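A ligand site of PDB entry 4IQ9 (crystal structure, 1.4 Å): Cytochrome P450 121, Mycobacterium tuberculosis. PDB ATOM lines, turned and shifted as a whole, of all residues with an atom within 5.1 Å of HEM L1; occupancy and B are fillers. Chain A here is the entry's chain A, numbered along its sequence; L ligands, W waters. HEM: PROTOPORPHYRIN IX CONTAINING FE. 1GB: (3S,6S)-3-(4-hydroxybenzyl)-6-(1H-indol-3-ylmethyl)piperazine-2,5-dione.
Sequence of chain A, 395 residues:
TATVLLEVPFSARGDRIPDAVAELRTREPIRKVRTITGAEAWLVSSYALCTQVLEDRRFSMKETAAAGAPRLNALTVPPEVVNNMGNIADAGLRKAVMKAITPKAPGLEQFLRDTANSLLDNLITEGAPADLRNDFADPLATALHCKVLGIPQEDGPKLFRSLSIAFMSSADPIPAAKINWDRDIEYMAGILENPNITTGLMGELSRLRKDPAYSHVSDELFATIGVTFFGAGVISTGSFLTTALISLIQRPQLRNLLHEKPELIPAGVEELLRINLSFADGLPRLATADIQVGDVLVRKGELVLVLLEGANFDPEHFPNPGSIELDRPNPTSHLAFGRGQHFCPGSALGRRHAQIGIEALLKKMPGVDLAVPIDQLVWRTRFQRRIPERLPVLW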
ATOM      1  N   LEU A  54       7.812 -14.117   5.631  1.00  0.00           N
ATOM      2  CA  LEU A  54       8.688 -14.472   4.510  1.00  0.00           C
ATOM      3  C   LEU A  54       8.357 -13.722   3.211  1.00  0.00           C
ATOM      4  O   LEU A  54       9.249 -13.540   2.388  1.00  0.00           O
ATOM      5  CB  LEU A  54       8.681 -15.980   4.277  1.00  0.00           C
ATOM      6  CG  LEU A  54       9.298 -16.819   5.416  1.00  0.00           C
ATOM      7  CD1 LEU A  54       9.180 -18.302   5.097  1.00  0.00           C
ATOM      8  CD2 LEU A  54      10.774 -16.447   5.661  1.00  0.00           C
ATOM      9  N   MET A  61      16.677 -10.378   5.430  1.00  0.00           N
ATOM     10  CA  MET A  61      17.717 -11.352   5.762  1.00  0.00           C
ATOM     11  C   MET A  61      19.056 -10.584   5.848  1.00  0.00           C
ATOM     12  O   MET A  61      19.828 -10.771   6.786  1.00  0.00           O
ATOM     13  CB  MET A  61      17.812 -12.468   4.694  1.00  0.00           C
ATOM     14  CG  MET A  61      19.167 -13.293   4.752  1.00  0.00           C
ATOM     15  SD  MET A  61      19.384 -14.458   3.375  1.00  0.00           S
ATOM     16  CE  MET A  61      18.131 -15.598   3.770  1.00  0.00           C
ATOM     17  N   ASN A  84      24.510 -13.327   0.186  1.00  0.00           N
ATOM     18  CA  ASN A  84      25.099 -14.011  -0.954  1.00  0.00           C
ATOM     19  C   ASN A  84      24.243 -14.019  -2.219  1.00  0.00           C
ATOM     20  O   ASN A  84      24.727 -13.660  -3.302  1.00  0.00           O
ATOM     21  CB  ASN A  84      25.453 -15.433  -0.517  1.00  0.00           C
ATOM     22  CG  ASN A  84      26.309 -16.197  -1.480  1.00  0.00           C
ATOM     23  OD1 ASN A  84      27.306 -15.697  -2.008  1.00  0.00           O
ATOM     24  ND2 ASN A  84      25.969 -17.483  -1.651  1.00  0.00           N
ATOM     25  N   MET A  85      22.968 -14.421  -2.104  1.00  0.00           N
ATOM     26  CA  MET A  85      22.113 -14.458  -3.288  1.00  0.00           C
ATOM     27  C   MET A  85      21.866 -13.104  -3.896  1.00  0.00           C
ATOM     28  O   MET A  85      21.867 -12.976  -5.126  1.00  0.00           O
ATOM     29  CB  MET A  85      20.809 -15.169  -3.012  1.00  0.00           C
ATOM     30  CG  MET A  85      20.931 -16.652  -3.195  1.00  0.00           C
ATOM     31  SD  MET A  85      21.310 -17.348  -4.843  1.00  0.00           S
ATOM     32  CE  MET A  85      20.733 -16.058  -5.984  1.00  0.00           C
ATOM     33  N   ILE A 101      22.765 -25.536 -11.448  1.00  0.00           N
ATOM     34  CA  ILE A 101      22.362 -26.391 -10.338  1.00  0.00           C
ATOM     35  C   ILE A 101      21.048 -27.166 -10.571  1.00  0.00           C
ATOM     36  O   ILE A 101      20.523 -27.755  -9.608  1.00  0.00           O
ATOM     37  CB  ILE A 101      22.444 -25.652  -8.978  1.00  0.00           C
ATOM     38  CG1 ILE A 101      21.343 -24.576  -8.872  1.00  0.00           C
ATOM     39  CG2 ILE A 101      23.854 -25.058  -8.728  1.00  0.00           C
ATOM     40  CD1 ILE A 101      21.211 -23.890  -7.517  1.00  0.00           C
ATOM     41  N   HIS A 145      27.419 -32.756  -5.283  1.00  0.00           N
ATOM     42  CA  HIS A 145      27.899 -31.386  -5.358  1.00  0.00           C
ATOM     43  C   HIS A 145      29.228 -31.208  -6.033  1.00  0.00           C
ATOM     44  O   HIS A 145      29.418 -30.188  -6.700  1.00  0.00           O
ATOM     45  CB  HIS A 145      27.754 -30.652  -4.030  1.00  0.00           C
ATOM     46  CG  HIS A 145      26.308 -30.405  -3.687  1.00  0.00           C
ATOM     47  ND1 HIS A 145      25.488 -31.416  -3.204  1.00  0.00           N
ATOM     48  CD2 HIS A 145      25.574 -29.272  -3.832  1.00  0.00           C
ATOM     49  CE1 HIS A 145      24.277 -30.877  -3.086  1.00  0.00           C
ATOM     50  NE2 HIS A 145      24.282 -29.577  -3.442  1.00  0.00           N
ATOM     51  N   PHE A 229      27.737 -22.548  -2.234  1.00  0.00           N
ATOM     52  CA  PHE A 229      26.823 -23.519  -2.854  1.00  0.00           C
ATOM     53  C   PHE A 229      27.218 -24.946  -2.505  1.00  0.00           C
ATOM     54  O   PHE A 229      26.329 -25.768  -2.243  1.00  0.00           O
ATOM     55  CB  PHE A 229      26.672 -23.267  -4.373  1.00  0.00           C
ATOM     56  CG  PHE A 229      25.618 -22.202  -4.624  1.00  0.00           C
ATOM     57  CD1 PHE A 229      25.810 -20.893  -4.216  1.00  0.00           C
ATOM     58  CD2 PHE A 229      24.411 -22.543  -5.220  1.00  0.00           C
ATOM     59  CE1 PHE A 229      24.817 -19.921  -4.402  1.00  0.00           C
ATOM     60  CE2 PHE A 229      23.400 -21.571  -5.389  1.00  0.00           C
ATOM     61  CZ  PHE A 229      23.625 -20.270  -5.012  1.00  0.00           C
ATOM     62  N   ALA A 232      26.123 -25.111   1.547  1.00  0.00           N
ATOM     63  CA  ALA A 232      24.669 -25.091   1.769  1.00  0.00           C
ATOM     64  C   ALA A 232      24.008 -26.305   1.097  1.00  0.00           C
ATOM     65  O   ALA A 232      23.159 -26.955   1.717  1.00  0.00           O
ATOM     66  CB  ALA A 232      24.056 -23.808   1.221  1.00  0.00           C
ATOM     67  N   GLY A 233      24.432 -26.646  -0.116  1.00  0.00           N
ATOM     68  CA  GLY A 233      23.817 -27.778  -0.800  1.00  0.00           C
ATOM     69  C   GLY A 233      24.114 -29.101  -0.119  1.00  0.00           C
ATOM     70  O   GLY A 233      23.197 -29.925   0.077  1.00  0.00           O
ATOM     71  N   SER A 236      22.436 -29.341   3.398  1.00  0.00           N
ATOM     72  CA  SER A 236      20.982 -29.396   3.336  1.00  0.00           C
ATOM     73  C   SER A 236      20.477 -30.705   2.762  1.00  0.00           C
ATOM     74  O   SER A 236      19.526 -31.292   3.327  1.00  0.00           O
ATOM     75  CB  SER A 236      20.424 -28.220   2.546  1.00  0.00           C
ATOM     76  OG  SER A 236      20.812 -26.975   3.129  1.00  0.00           O
ATOM     77  N   THR A 237      21.096 -31.194   1.656  1.00  0.00           N
ATOM     78  CA  THR A 237      20.656 -32.444   1.049  1.00  0.00           C
ATOM     79  C   THR A 237      21.051 -33.643   1.907  1.00  0.00           C
ATOM     80  O   THR A 237      20.241 -34.553   2.087  1.00  0.00           O
ATOM     81  CB  THR A 237      21.161 -32.595  -0.393  1.00  0.00           C
ATOM     82  OG1 THR A 237      22.605 -32.549  -0.401  1.00  0.00           O
ATOM     83  CG2 THR A 237      20.560 -31.537  -1.326  1.00  0.00           C
ATOM     84  N   PHE A 240      18.697 -33.477   5.053  1.00  0.00           N
ATOM     85  CA  PHE A 240      17.299 -33.800   4.751  1.00  0.00           C
ATOM     86  C   PHE A 240      17.155 -35.274   4.406  1.00  0.00           C
ATOM     87  O   PHE A 240      16.266 -35.925   4.954  1.00  0.00           O
ATOM     88  CB  PHE A 240      16.755 -32.928   3.603  1.00  0.00           C
ATOM     89  CG  PHE A 240      15.425 -33.453   3.151  1.00  0.00           C
ATOM     90  CD1 PHE A 240      14.342 -33.471   4.033  1.00  0.00           C
ATOM     91  CD2 PHE A 240      15.276 -34.056   1.901  1.00  0.00           C
ATOM     92  CE1 PHE A 240      13.127 -34.067   3.655  1.00  0.00           C
ATOM     93  CE2 PHE A 240      14.056 -34.638   1.532  1.00  0.00           C
ATOM     94  CZ  PHE A 240      12.998 -34.651   2.416  1.00  0.00           C
ATOM     95  N   LEU A 273       9.405 -33.822   2.936  1.00  0.00           N
ATOM     96  CA  LEU A 273       9.874 -32.435   3.054  1.00  0.00           C
ATOM     97  C   LEU A 273       8.939 -31.667   3.999  1.00  0.00           C
ATOM     98  O   LEU A 273       9.402 -30.951   4.886  1.00  0.00           O
ATOM     99  CB  LEU A 273       9.892 -31.754   1.678  1.00  0.00           C
ATOM    100  CG  LEU A 273      11.079 -32.106   0.798  1.00  0.00           C
ATOM    101  CD1 LEU A 273      10.788 -31.768  -0.661  1.00  0.00           C
ATOM    102  CD2 LEU A 273      12.341 -31.360   1.247  1.00  0.00           C
ATOM    103  N   ASN A 276       9.548 -32.505   7.619  1.00  0.00           N
ATOM    104  CA  ASN A 276      10.973 -32.538   7.978  1.00  0.00           C
ATOM    105  C   ASN A 276      11.330 -31.574   9.104  1.00  0.00           C
ATOM    106  O   ASN A 276      10.890 -30.418   9.106  1.00  0.00           O
ATOM    107  CB  ASN A 276      11.852 -32.362   6.731  1.00  0.00           C
ATOM    108  CG  ASN A 276      12.482 -31.002   6.534  1.00  0.00           C
ATOM    109  OD1 ASN A 276      13.480 -30.678   7.181  1.00  0.00           O
ATOM    110  ND2 ASN A 276      11.961 -30.166   5.612  1.00  0.00           N
ATOM    111  N   PHE A 279      15.731 -28.188   9.756  1.00  0.00           N
ATOM    112  CA  PHE A 279      16.197 -26.856  10.188  1.00  0.00           C
ATOM    113  C   PHE A 279      16.049 -26.756  11.695  1.00  0.00           C
ATOM    114  O   PHE A 279      14.956 -26.866  12.225  1.00  0.00           O
ATOM    115  CB  PHE A 279      15.451 -25.726   9.447  1.00  0.00           C
ATOM    116  CG  PHE A 279      16.093 -25.336   8.135  1.00  0.00           C
ATOM    117  CD1 PHE A 279      16.134 -26.231   7.079  1.00  0.00           C
ATOM    118  CD2 PHE A 279      16.682 -24.094   7.977  1.00  0.00           C
ATOM    119  CE1 PHE A 279      16.768 -25.882   5.875  1.00  0.00           C
ATOM    120  CE2 PHE A 279      17.275 -23.728   6.761  1.00  0.00           C
ATOM    121  CZ  PHE A 279      17.330 -24.638   5.736  1.00  0.00           C
ATOM    122  N   LEU A 283      13.950 -19.374  10.719  1.00  0.00           N
ATOM    123  CA  LEU A 283      14.680 -18.551   9.746  1.00  0.00           C
ATOM    124  C   LEU A 283      14.712 -17.125  10.267  1.00  0.00           C
ATOM    125  O   LEU A 283      13.659 -16.564  10.596  1.00  0.00           O
ATOM    126  CB  LEU A 283      13.981 -18.565   8.377  1.00  0.00           C
ATOM    127  CG  LEU A 283      13.765 -19.928   7.731  1.00  0.00           C
ATOM    128  CD1 LEU A 283      13.114 -19.745   6.380  1.00  0.00           C
ATOM    129  CD2 LEU A 283      15.115 -20.714   7.589  1.00  0.00           C
ATOM    130  N   PRO A 284      15.911 -16.522  10.402  1.00  0.00           N
ATOM    131  CA  PRO A 284      15.967 -15.177  10.996  1.00  0.00           C
ATOM    132  C   PRO A 284      15.760 -14.058   9.997  1.00  0.00           C
ATOM    133  O   PRO A 284      16.229 -14.113   8.847  1.00  0.00           O
ATOM    134  CB  PRO A 284      17.386 -15.116  11.594  1.00  0.00           C
ATOM    135  CG  PRO A 284      18.202 -16.029  10.709  1.00  0.00           C
ATOM    136  CD  PRO A 284      17.251 -17.113  10.221  1.00  0.00           C
ATOM    137  N   ARG A 285      15.094 -12.994  10.468  1.00  0.00           N
ATOM    138  CA  ARG A 285      14.871 -11.761   9.728  1.00  0.00           C
ATOM    139  C   ARG A 285      14.942 -10.597  10.701  1.00  0.00           C
ATOM    140  O   ARG A 285      14.544 -10.728  11.867  1.00  0.00           O
ATOM    141  CB  ARG A 285      13.468 -11.743   9.087  1.00  0.00           C
ATOM    142  CG  ARG A 285      13.237 -12.829   8.021  1.00  0.00           C
ATOM    143  CD  ARG A 285      14.094 -12.632   6.787  1.00  0.00           C
ATOM    144  NE  ARG A 285      13.712 -13.521   5.675  1.00  0.00           N
ATOM    145  CZ  ARG A 285      14.258 -14.708   5.409  1.00  0.00           C
ATOM    146  NH1 ARG A 285      15.194 -15.213   6.211  1.00  0.00           N
ATOM    147  NH2 ARG A 285      13.865 -15.391   4.331  1.00  0.00           N
ATOM    148  N   LEU A 308       9.823 -23.119  10.720  1.00  0.00           N
ATOM    149  CA  LEU A 308       9.292 -23.873   9.573  1.00  0.00           C
ATOM    150  C   LEU A 308       8.329 -24.982   9.964  1.00  0.00           C
ATOM    151  O   LEU A 308       7.297 -25.163   9.298  1.00  0.00           O
ATOM    152  CB  LEU A 308      10.412 -24.409   8.669  1.00  0.00           C
ATOM    153  CG  LEU A 308      11.338 -23.336   8.051  1.00  0.00           C
ATOM    154  CD1 LEU A 308      12.398 -23.969   7.166  1.00  0.00           C
ATOM    155  CD2 LEU A 308      10.542 -22.284   7.258  1.00  0.00           C
ATOM    156  N   LEU A 335       6.681 -24.991   3.579  1.00  0.00           N
ATOM    157  CA  LEU A 335       7.774 -24.022   3.627  1.00  0.00           C
ATOM    158  C   LEU A 335       9.142 -24.674   3.805  1.00  0.00           C
ATOM    159  O   LEU A 335      10.076 -24.004   4.259  1.00  0.00           O
ATOM    160  CB  LEU A 335       7.529 -23.003   4.744  1.00  0.00           C
ATOM    161  CG  LEU A 335       6.180 -22.260   4.777  1.00  0.00           C
ATOM    162  CD1 LEU A 335       6.244 -21.139   5.782  1.00  0.00           C
ATOM    163  CD2 LEU A 335       5.756 -21.717   3.424  1.00  0.00           C
ATOM    164  N   ALA A 336       9.303 -25.972   3.408  1.00  0.00           N
ATOM    165  CA  ALA A 336      10.619 -26.613   3.579  1.00  0.00           C
ATOM    166  C   ALA A 336      11.745 -25.919   2.838  1.00  0.00           C
ATOM    167  O   ALA A 336      12.894 -26.021   3.270  1.00  0.00           O
ATOM    168  CB  ALA A 336      10.566 -28.064   3.135  1.00  0.00           C
ATOM    169  N   PHE A 337      11.439 -25.230   1.716  1.00  0.00           N
ATOM    170  CA  PHE A 337      12.431 -24.482   0.932  1.00  0.00           C
ATOM    171  C   PHE A 337      12.260 -22.977   1.148  1.00  0.00           C
ATOM    172  O   PHE A 337      12.814 -22.188   0.379  1.00  0.00           O
ATOM    173  CB  PHE A 337      12.301 -24.833  -0.571  1.00  0.00           C
ATOM    174  CG  PHE A 337      12.643 -26.279  -0.876  1.00  0.00           C
ATOM    175  CD1 PHE A 337      13.943 -26.758  -0.681  1.00  0.00           C
ATOM    176  CD2 PHE A 337      11.698 -27.129  -1.438  1.00  0.00           C
ATOM    177  CE1 PHE A 337      14.274 -28.081  -0.977  1.00  0.00           C
ATOM    178  CE2 PHE A 337      12.034 -28.449  -1.757  1.00  0.00           C
ATOM    179  CZ  PHE A 337      13.316 -28.920  -1.515  1.00  0.00           C
ATOM    180  N   GLY A 338      11.540 -22.579   2.188  1.00  0.00           N
ATOM    181  CA  GLY A 338      11.277 -21.157   2.408  1.00  0.00           C
ATOM    182  C   GLY A 338      10.138 -20.653   1.533  1.00  0.00           C
ATOM    183  O   GLY A 338       9.315 -21.425   1.011  1.00  0.00           O
ATOM    184  N   GLN A 341      11.425 -13.859  -1.386  1.00  0.00           N
ATOM    185  CA  GLN A 341      12.693 -13.403  -1.940  1.00  0.00           C
ATOM    186  C   GLN A 341      13.821 -14.433  -1.828  1.00  0.00           C
ATOM    187  O   GLN A 341      14.633 -14.542  -2.756  1.00  0.00           O
ATOM    188  CB  GLN A 341      13.095 -12.075  -1.283  1.00  0.00           C
ATOM    189  CG  GLN A 341      14.400 -11.436  -1.802  1.00  0.00           C
ATOM    190  CD  GLN A 341      14.315 -10.902  -3.220  1.00  0.00           C
ATOM    191  OE1 GLN A 341      15.339 -10.624  -3.860  1.00  0.00           O
ATOM    192  NE2 GLN A 341      13.120 -10.715  -3.730  1.00  0.00           N
ATOM    193  N   HIS A 342      13.866 -15.161  -0.699  1.00  0.00           N
ATOM    194  CA  HIS A 342      14.962 -16.072  -0.399  1.00  0.00           C
ATOM    195  C   HIS A 342      14.645 -17.532  -0.594  1.00  0.00           C
ATOM    196  O   HIS A 342      15.372 -18.397  -0.097  1.00  0.00           O
ATOM    197  CB  HIS A 342      15.526 -15.769   0.995  1.00  0.00           C
ATOM    198  CG  HIS A 342      16.069 -14.373   1.098  1.00  0.00           C
ATOM    199  ND1 HIS A 342      17.309 -14.038   0.547  1.00  0.00           N
ATOM    200  CD2 HIS A 342      15.510 -13.257   1.620  1.00  0.00           C
ATOM    201  CE1 HIS A 342      17.446 -12.735   0.748  1.00  0.00           C
ATOM    202  NE2 HIS A 342      16.405 -12.228   1.408  1.00  0.00           N
ATOM    203  N   PHE A 343      13.585 -17.830  -1.387  1.00  0.00           N
ATOM    204  CA  PHE A 343      13.207 -19.222  -1.695  1.00  0.00           C
ATOM    205  C   PHE A 343      14.442 -19.979  -2.203  1.00  0.00           C
ATOM    206  O   PHE A 343      15.191 -19.465  -3.040  1.00  0.00           O
ATOM    207  CB  PHE A 343      12.086 -19.223  -2.736  1.00  0.00           C
ATOM    208  CG  PHE A 343      11.593 -20.615  -3.071  1.00  0.00           C
ATOM    209  CD1 PHE A 343      10.676 -21.263  -2.247  1.00  0.00           C
ATOM    210  CD2 PHE A 343      12.095 -21.305  -4.159  1.00  0.00           C
ATOM    211  CE1 PHE A 343      10.233 -22.569  -2.541  1.00  0.00           C
ATOM    212  CE2 PHE A 343      11.698 -22.625  -4.423  1.00  0.00           C
ATOM    213  CZ  PHE A 343      10.767 -23.240  -3.612  1.00  0.00           C
ATOM    214  N   CYS A 344      14.650 -21.188  -1.678  1.00  0.00           N
ATOM    215  CA  CYS A 344      15.820 -21.983  -2.007  1.00  0.00           C
ATOM    216  C   CYS A 344      16.083 -22.100  -3.505  1.00  0.00           C
ATOM    217  O   CYS A 344      15.265 -22.697  -4.195  1.00  0.00           O
ATOM    218  CB  CYS A 344      15.706 -23.358  -1.384  1.00  0.00           C
ATOM    219  SG  CYS A 344      17.156 -24.410  -1.684  1.00  0.00           S
ATOM    220  N   PRO A 345      17.285 -21.718  -3.968  1.00  0.00           N
ATOM    221  CA  PRO A 345      17.589 -21.891  -5.404  1.00  0.00           C
ATOM    222  C   PRO A 345      17.924 -23.343  -5.770  1.00  0.00           C
ATOM    223  O   PRO A 345      17.930 -23.680  -6.966  1.00  0.00           O
ATOM    224  CB  PRO A 345      18.795 -20.965  -5.620  1.00  0.00           C
ATOM    225  CG  PRO A 345      19.487 -20.940  -4.294  1.00  0.00           C
ATOM    226  CD  PRO A 345      18.371 -21.012  -3.260  1.00  0.00           C
ATOM    227  N   GLY A 346      18.180 -24.186  -4.771  1.00  0.00           N
ATOM    228  CA  GLY A 346      18.508 -25.589  -5.016  1.00  0.00           C
ATOM    229  C   GLY A 346      17.335 -26.530  -4.818  1.00  0.00           C
ATOM    230  O   GLY A 346      17.552 -27.742  -4.768  1.00  0.00           O
ATOM    231  N   LEU A 349      17.091 -29.562  -7.233  1.00  0.00           N
ATOM    232  CA  LEU A 349      18.199 -30.502  -7.016  1.00  0.00           C
ATOM    233  C   LEU A 349      18.022 -31.290  -5.705  1.00  0.00           C
ATOM    234  O   LEU A 349      18.319 -32.482  -5.664  1.00  0.00           O
ATOM    235  CB  LEU A 349      19.531 -29.741  -7.034  1.00  0.00           C
ATOM    236  CG  LEU A 349      20.820 -30.563  -6.987  1.00  0.00           C
ATOM    237  CD1 LEU A 349      20.981 -31.431  -8.248  1.00  0.00           C
ATOM    238  CD2 LEU A 349      22.032 -29.670  -6.843  1.00  0.00           C
ATOM    239  N   GLY A 350      17.577 -30.609  -4.633  1.00  0.00           N
ATOM    240  CA  GLY A 350      17.336 -31.264  -3.362  1.00  0.00           C
ATOM    241  C   GLY A 350      16.250 -32.305  -3.461  1.00  0.00           C
ATOM    242  O   GLY A 350      16.382 -33.401  -2.915  1.00  0.00           O
HETATM  243  CHA HEM L   1      18.024 -21.096   1.025  1.00  0.00           C
HETATM  244  CHB HEM L   1      16.144 -25.352   2.433  1.00  0.00           C
HETATM  245  CHC HEM L   1      19.042 -27.572  -0.793  1.00  0.00           C
HETATM  246  CHD HEM L   1      21.324 -23.381  -1.641  1.00  0.00           C
HETATM  247  C1A HEM L   1      17.187 -22.047   1.620  1.00  0.00           C
HETATM  248  C2A HEM L   1      16.095 -21.771   2.506  1.00  0.00           C
HETATM  249  C3A HEM L   1      15.618 -22.957   2.948  1.00  0.00           C
HETATM  250  C4A HEM L   1      16.357 -23.979   2.283  1.00  0.00           C
HETATM  251  CMA HEM L   1      14.485 -23.202   3.928  1.00  0.00           C
HETATM  252  CAA HEM L   1      15.571 -20.392   2.864  1.00  0.00           C
HETATM  253  CBA HEM L   1      16.406 -19.682   3.942  1.00  0.00           C
HETATM  254  CGA HEM L   1      15.775 -18.368   4.348  1.00  0.00           C
HETATM  255  O1A HEM L   1      14.848 -17.860   3.704  1.00  0.00           O
HETATM  256  O2A HEM L   1      16.324 -17.808   5.434  1.00  0.00           O
HETATM  257  C1B HEM L   1      16.865 -26.352   1.715  1.00  0.00           C
HETATM  258  C2B HEM L   1      16.527 -27.750   1.782  1.00  0.00           C
HETATM  259  C3B HEM L   1      17.305 -28.379   0.848  1.00  0.00           C
HETATM  260  C4B HEM L   1      18.140 -27.307   0.260  1.00  0.00           C
HETATM  261  CMB HEM L   1      15.495 -28.361   2.700  1.00  0.00           C
HETATM  262  CAB HEM L   1      17.387 -29.794   0.460  1.00  0.00           C
HETATM  263  CBB HEM L   1      16.605 -30.763   0.826  1.00  0.00           C
HETATM  264  C1C HEM L   1      19.876 -26.621  -1.354  1.00  0.00           C
HETATM  265  C2C HEM L   1      20.830 -26.898  -2.400  1.00  0.00           C
HETATM  266  C3C HEM L   1      21.530 -25.693  -2.586  1.00  0.00           C
HETATM  267  C4C HEM L   1      20.939 -24.705  -1.725  1.00  0.00           C
HETATM  268  CMC HEM L   1      21.039 -28.206  -3.110  1.00  0.00           C
HETATM  269  CAC HEM L   1      22.632 -25.392  -3.546  1.00  0.00           C
HETATM  270  CBC HEM L   1      23.332 -26.291  -4.268  1.00  0.00           C
HETATM  271  C1D HEM L   1      20.682 -22.433  -0.885  1.00  0.00           C
HETATM  272  C2D HEM L   1      21.048 -21.017  -0.868  1.00  0.00           C
HETATM  273  C3D HEM L   1      20.046 -20.353  -0.222  1.00  0.00           C
HETATM  274  C4D HEM L   1      19.132 -21.407   0.248  1.00  0.00           C
HETATM  275  CMD HEM L   1      22.289 -20.444  -1.556  1.00  0.00           C
HETATM  276  CAD HEM L   1      19.945 -18.847   0.056  1.00  0.00           C
HETATM  277  CBD HEM L   1      18.937 -18.201  -0.914  1.00  0.00           C
HETATM  278  CGD HEM L   1      18.657 -16.677  -0.764  1.00  0.00           C
HETATM  279  O1D HEM L   1      17.982 -16.151  -1.634  1.00  0.00           O
HETATM  280  O2D HEM L   1      19.186 -16.098   0.260  1.00  0.00           O
HETATM  281  NA  HEM L   1      17.328 -23.430   1.463  1.00  0.00           N
HETATM  282  NB  HEM L   1      17.866 -26.098   0.798  1.00  0.00           N
HETATM  283  NC  HEM L   1      19.903 -25.292  -0.983  1.00  0.00           N
HETATM  284  ND  HEM L   1      19.533 -22.630  -0.157  1.00  0.00           N
HETATM  285 FE   HEM L   1      18.573 -24.346   0.181  1.00  0.00          FE
HETATM  286  OB  1GB L   2      22.321 -18.417   7.648  1.00  0.00           O
HETATM  287  CB  1GB L   2      22.240 -19.371   6.828  1.00  0.00           C
HETATM  288  CAB 1GB L   2      23.354 -20.249   6.428  1.00  0.00           C
HETATM  289  CBB 1GB L   2      24.461 -19.353   5.735  1.00  0.00           C
HETATM  290  CGB 1GB L   2      25.783 -20.018   5.577  1.00  0.00           C
HETATM  291  CD4 1GB L   2      26.358 -20.325   4.361  1.00  0.00           C
HETATM  292  CE4 1GB L   2      27.584 -20.921   4.207  1.00  0.00           C
HETATM  293  CZB 1GB L   2      28.312 -21.284   5.454  1.00  0.00           C
HETATM  294  OHB 1GB L   2      29.508 -21.855   5.360  1.00  0.00           O
HETATM  295  CE3 1GB L   2      27.798 -21.030   6.727  1.00  0.00           C
HETATM  296  CD3 1GB L   2      26.509 -20.368   6.757  1.00  0.00           C
HETATM  297  NB  1GB L   2      22.983 -21.317   5.554  1.00  0.00           N
HETATM  298  CA  1GB L   2      21.864 -21.672   4.986  1.00  0.00           C
HETATM  299  OA  1GB L   2      21.828 -22.696   4.262  1.00  0.00           O
HETATM  300  NA  1GB L   2      20.953 -19.650   6.265  1.00  0.00           N
HETATM  301  CAA 1GB L   2      20.651 -20.732   5.297  1.00  0.00           C
HETATM  302  CBA 1GB L   2      20.204 -19.968   3.905  1.00  0.00           C
HETATM  303  CGA 1GB L   2      21.221 -18.920   3.467  1.00  0.00           C
HETATM  304  CD2 1GB L   2      22.366 -19.057   2.694  1.00  0.00           C
HETATM  305  CE2 1GB L   2      22.992 -20.157   2.029  1.00  0.00           C
HETATM  306  CZ3 1GB L   2      24.209 -19.955   1.267  1.00  0.00           C
HETATM  307  CH2 1GB L   2      24.786 -18.645   1.184  1.00  0.00           C
HETATM  308  CZ2 1GB L   2      24.124 -17.573   1.867  1.00  0.00           C
HETATM  309  CE1 1GB L   2      22.956 -17.764   2.600  1.00  0.00           C
HETATM  310  NE1 1GB L   2      22.223 -16.861   3.267  1.00  0.00           N
HETATM  311  CD1 1GB L   2      21.136 -17.549   3.812  1.00  0.00           C
HETATM  312  O   HOH W   1      16.941 -17.423  -3.769  1.00  0.00           O
HETATM  313  O   HOH W   2      17.358 -13.873  -3.143  1.00  0.00           O
HETATM  314  O   HOH W   3      21.631 -15.023   0.457  1.00  0.00           O
HETATM  315  O   HOH W   4      19.162 -23.000   3.940  1.00  0.00           O
HETATM  316  O   HOH W   5      12.665 -18.118   2.151  1.00  0.00           O
HETATM  317  O   HOH W   6      20.077 -24.496   1.945  1.00  0.00           O
HETATM  318  O   HOH W   7      18.500 -18.450   6.774  1.00  0.00           O
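A ring nitrogen (ND1) of His 342 is in hydrogen-bond range of the side-chain sulfur (SD) of Met 61, 3.5 Å away. N of Cys 344 lies within hydrogen-bond range of O of Phe 337, at 2.9 Å. O of Gly 233 sits at hydrogen-bond distance from OG1 of Thr 237, 2.7 Å away. The side-chain hydroxyl (OG) of Ser 236 is in hydrogen-bond range of the backbone carbonyl oxygen (O) of Ala 232 (2.7 Å). The side-chain sulfur (SG) of Cys 344 sits close to the backbone NH (N) of Gly 346.
Water W6 lies within hydrogen-bond range of OG of Ser 236 (2.8 Å) and OA of 1GB L2 (3.4 Å). Water W7 lies within hydrogen-bond range of O2A of HEM L1 (2.6 Å) and NA of 1GB L2 (2.8 Å). Water W1 lies within hydrogen-bond range of O1D of HEM L1 and O of Phe 343. Water W2 lies within hydrogen-bond range of O1D of HEM L1 (2.8 Å) and O of Gln 341 (2.8 Å).
The side-chain sulfur of Cys 344 is bound to an iron atom (FE) of HEM L1 (2.3 Å). An oxygen (O1A) of HEM L1 lies within salt-bridge range of the guanidinium group of Arg 285 (2.7 Å). ND1 of His 342 is in hydrogen-bond range of O2D of HEM L1, 2.8 Å away. The side-chain sulfur of Met 61 lies close to a nitrogen (NE1) of 1GB L2 (3.7 Å).
The side-chain sulfur of Met 61 sits close to an oxygen (O2D) of HEM L1 (3.5 Å). CB of Met 85 touches O1D of HEM L1 (3.3 Å). His 145 touches HEM L1. O of Phe 229 touches CBC of HEM L1 (3.7 Å). Ala 232 touches HEM L1. Gly 233 touches HEM L1 (CA to C2C, 3.5 Å). Ser 236 touches HEM L1 (CB to C4B, 3.4 Å). CG2 of Thr 237 touches CMC of HEM L1, 3.8 Å away. Phe 240 touches HEM L1 (CB to CBB, 3.5 Å). Phe 279 touches HEM L1 (CE1 to CHB, 3.5 Å). Leu 283 touches HEM L1 (CD1 to CGA, 3.6 Å). CD1 of Leu 308 touches CMA of HEM L1 (3.9 Å). Ala 336 touches HEM L1. Phe 337 touches HEM L1. Gly 338 touches HEM L1 (N to CMA, 3.5 Å). O of Gln 341 touches O1D of HEM L1, at 3.9 Å. Pro 345 touches HEM L1. Gly 346 touches HEM L1 (CA to C2C, 3.7 Å). Hydrophobic or aromatic side chains that line HEM L1: Met 61, Met 85, His 145, Phe 229, Ala 232, Phe 240, Phe 279, Leu 283, Leu 308, Phe 337, His 342 and Pro 345. Within 4 Å of HEM L1: Met 61, Met 85, His 145, Phe 229, Ala 232, Gly 233, Ser 236, Thr 237, Phe 240, Phe 279, Leu 283, Arg 285, Leu 308, Ala 336, Phe 337, Gly 338, Gln 341, His 342, Cys 344, Pro 345 and Gly 346. The nearest printed residue that does not touch HEM L1 is Gly 350 (4.1 Å).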
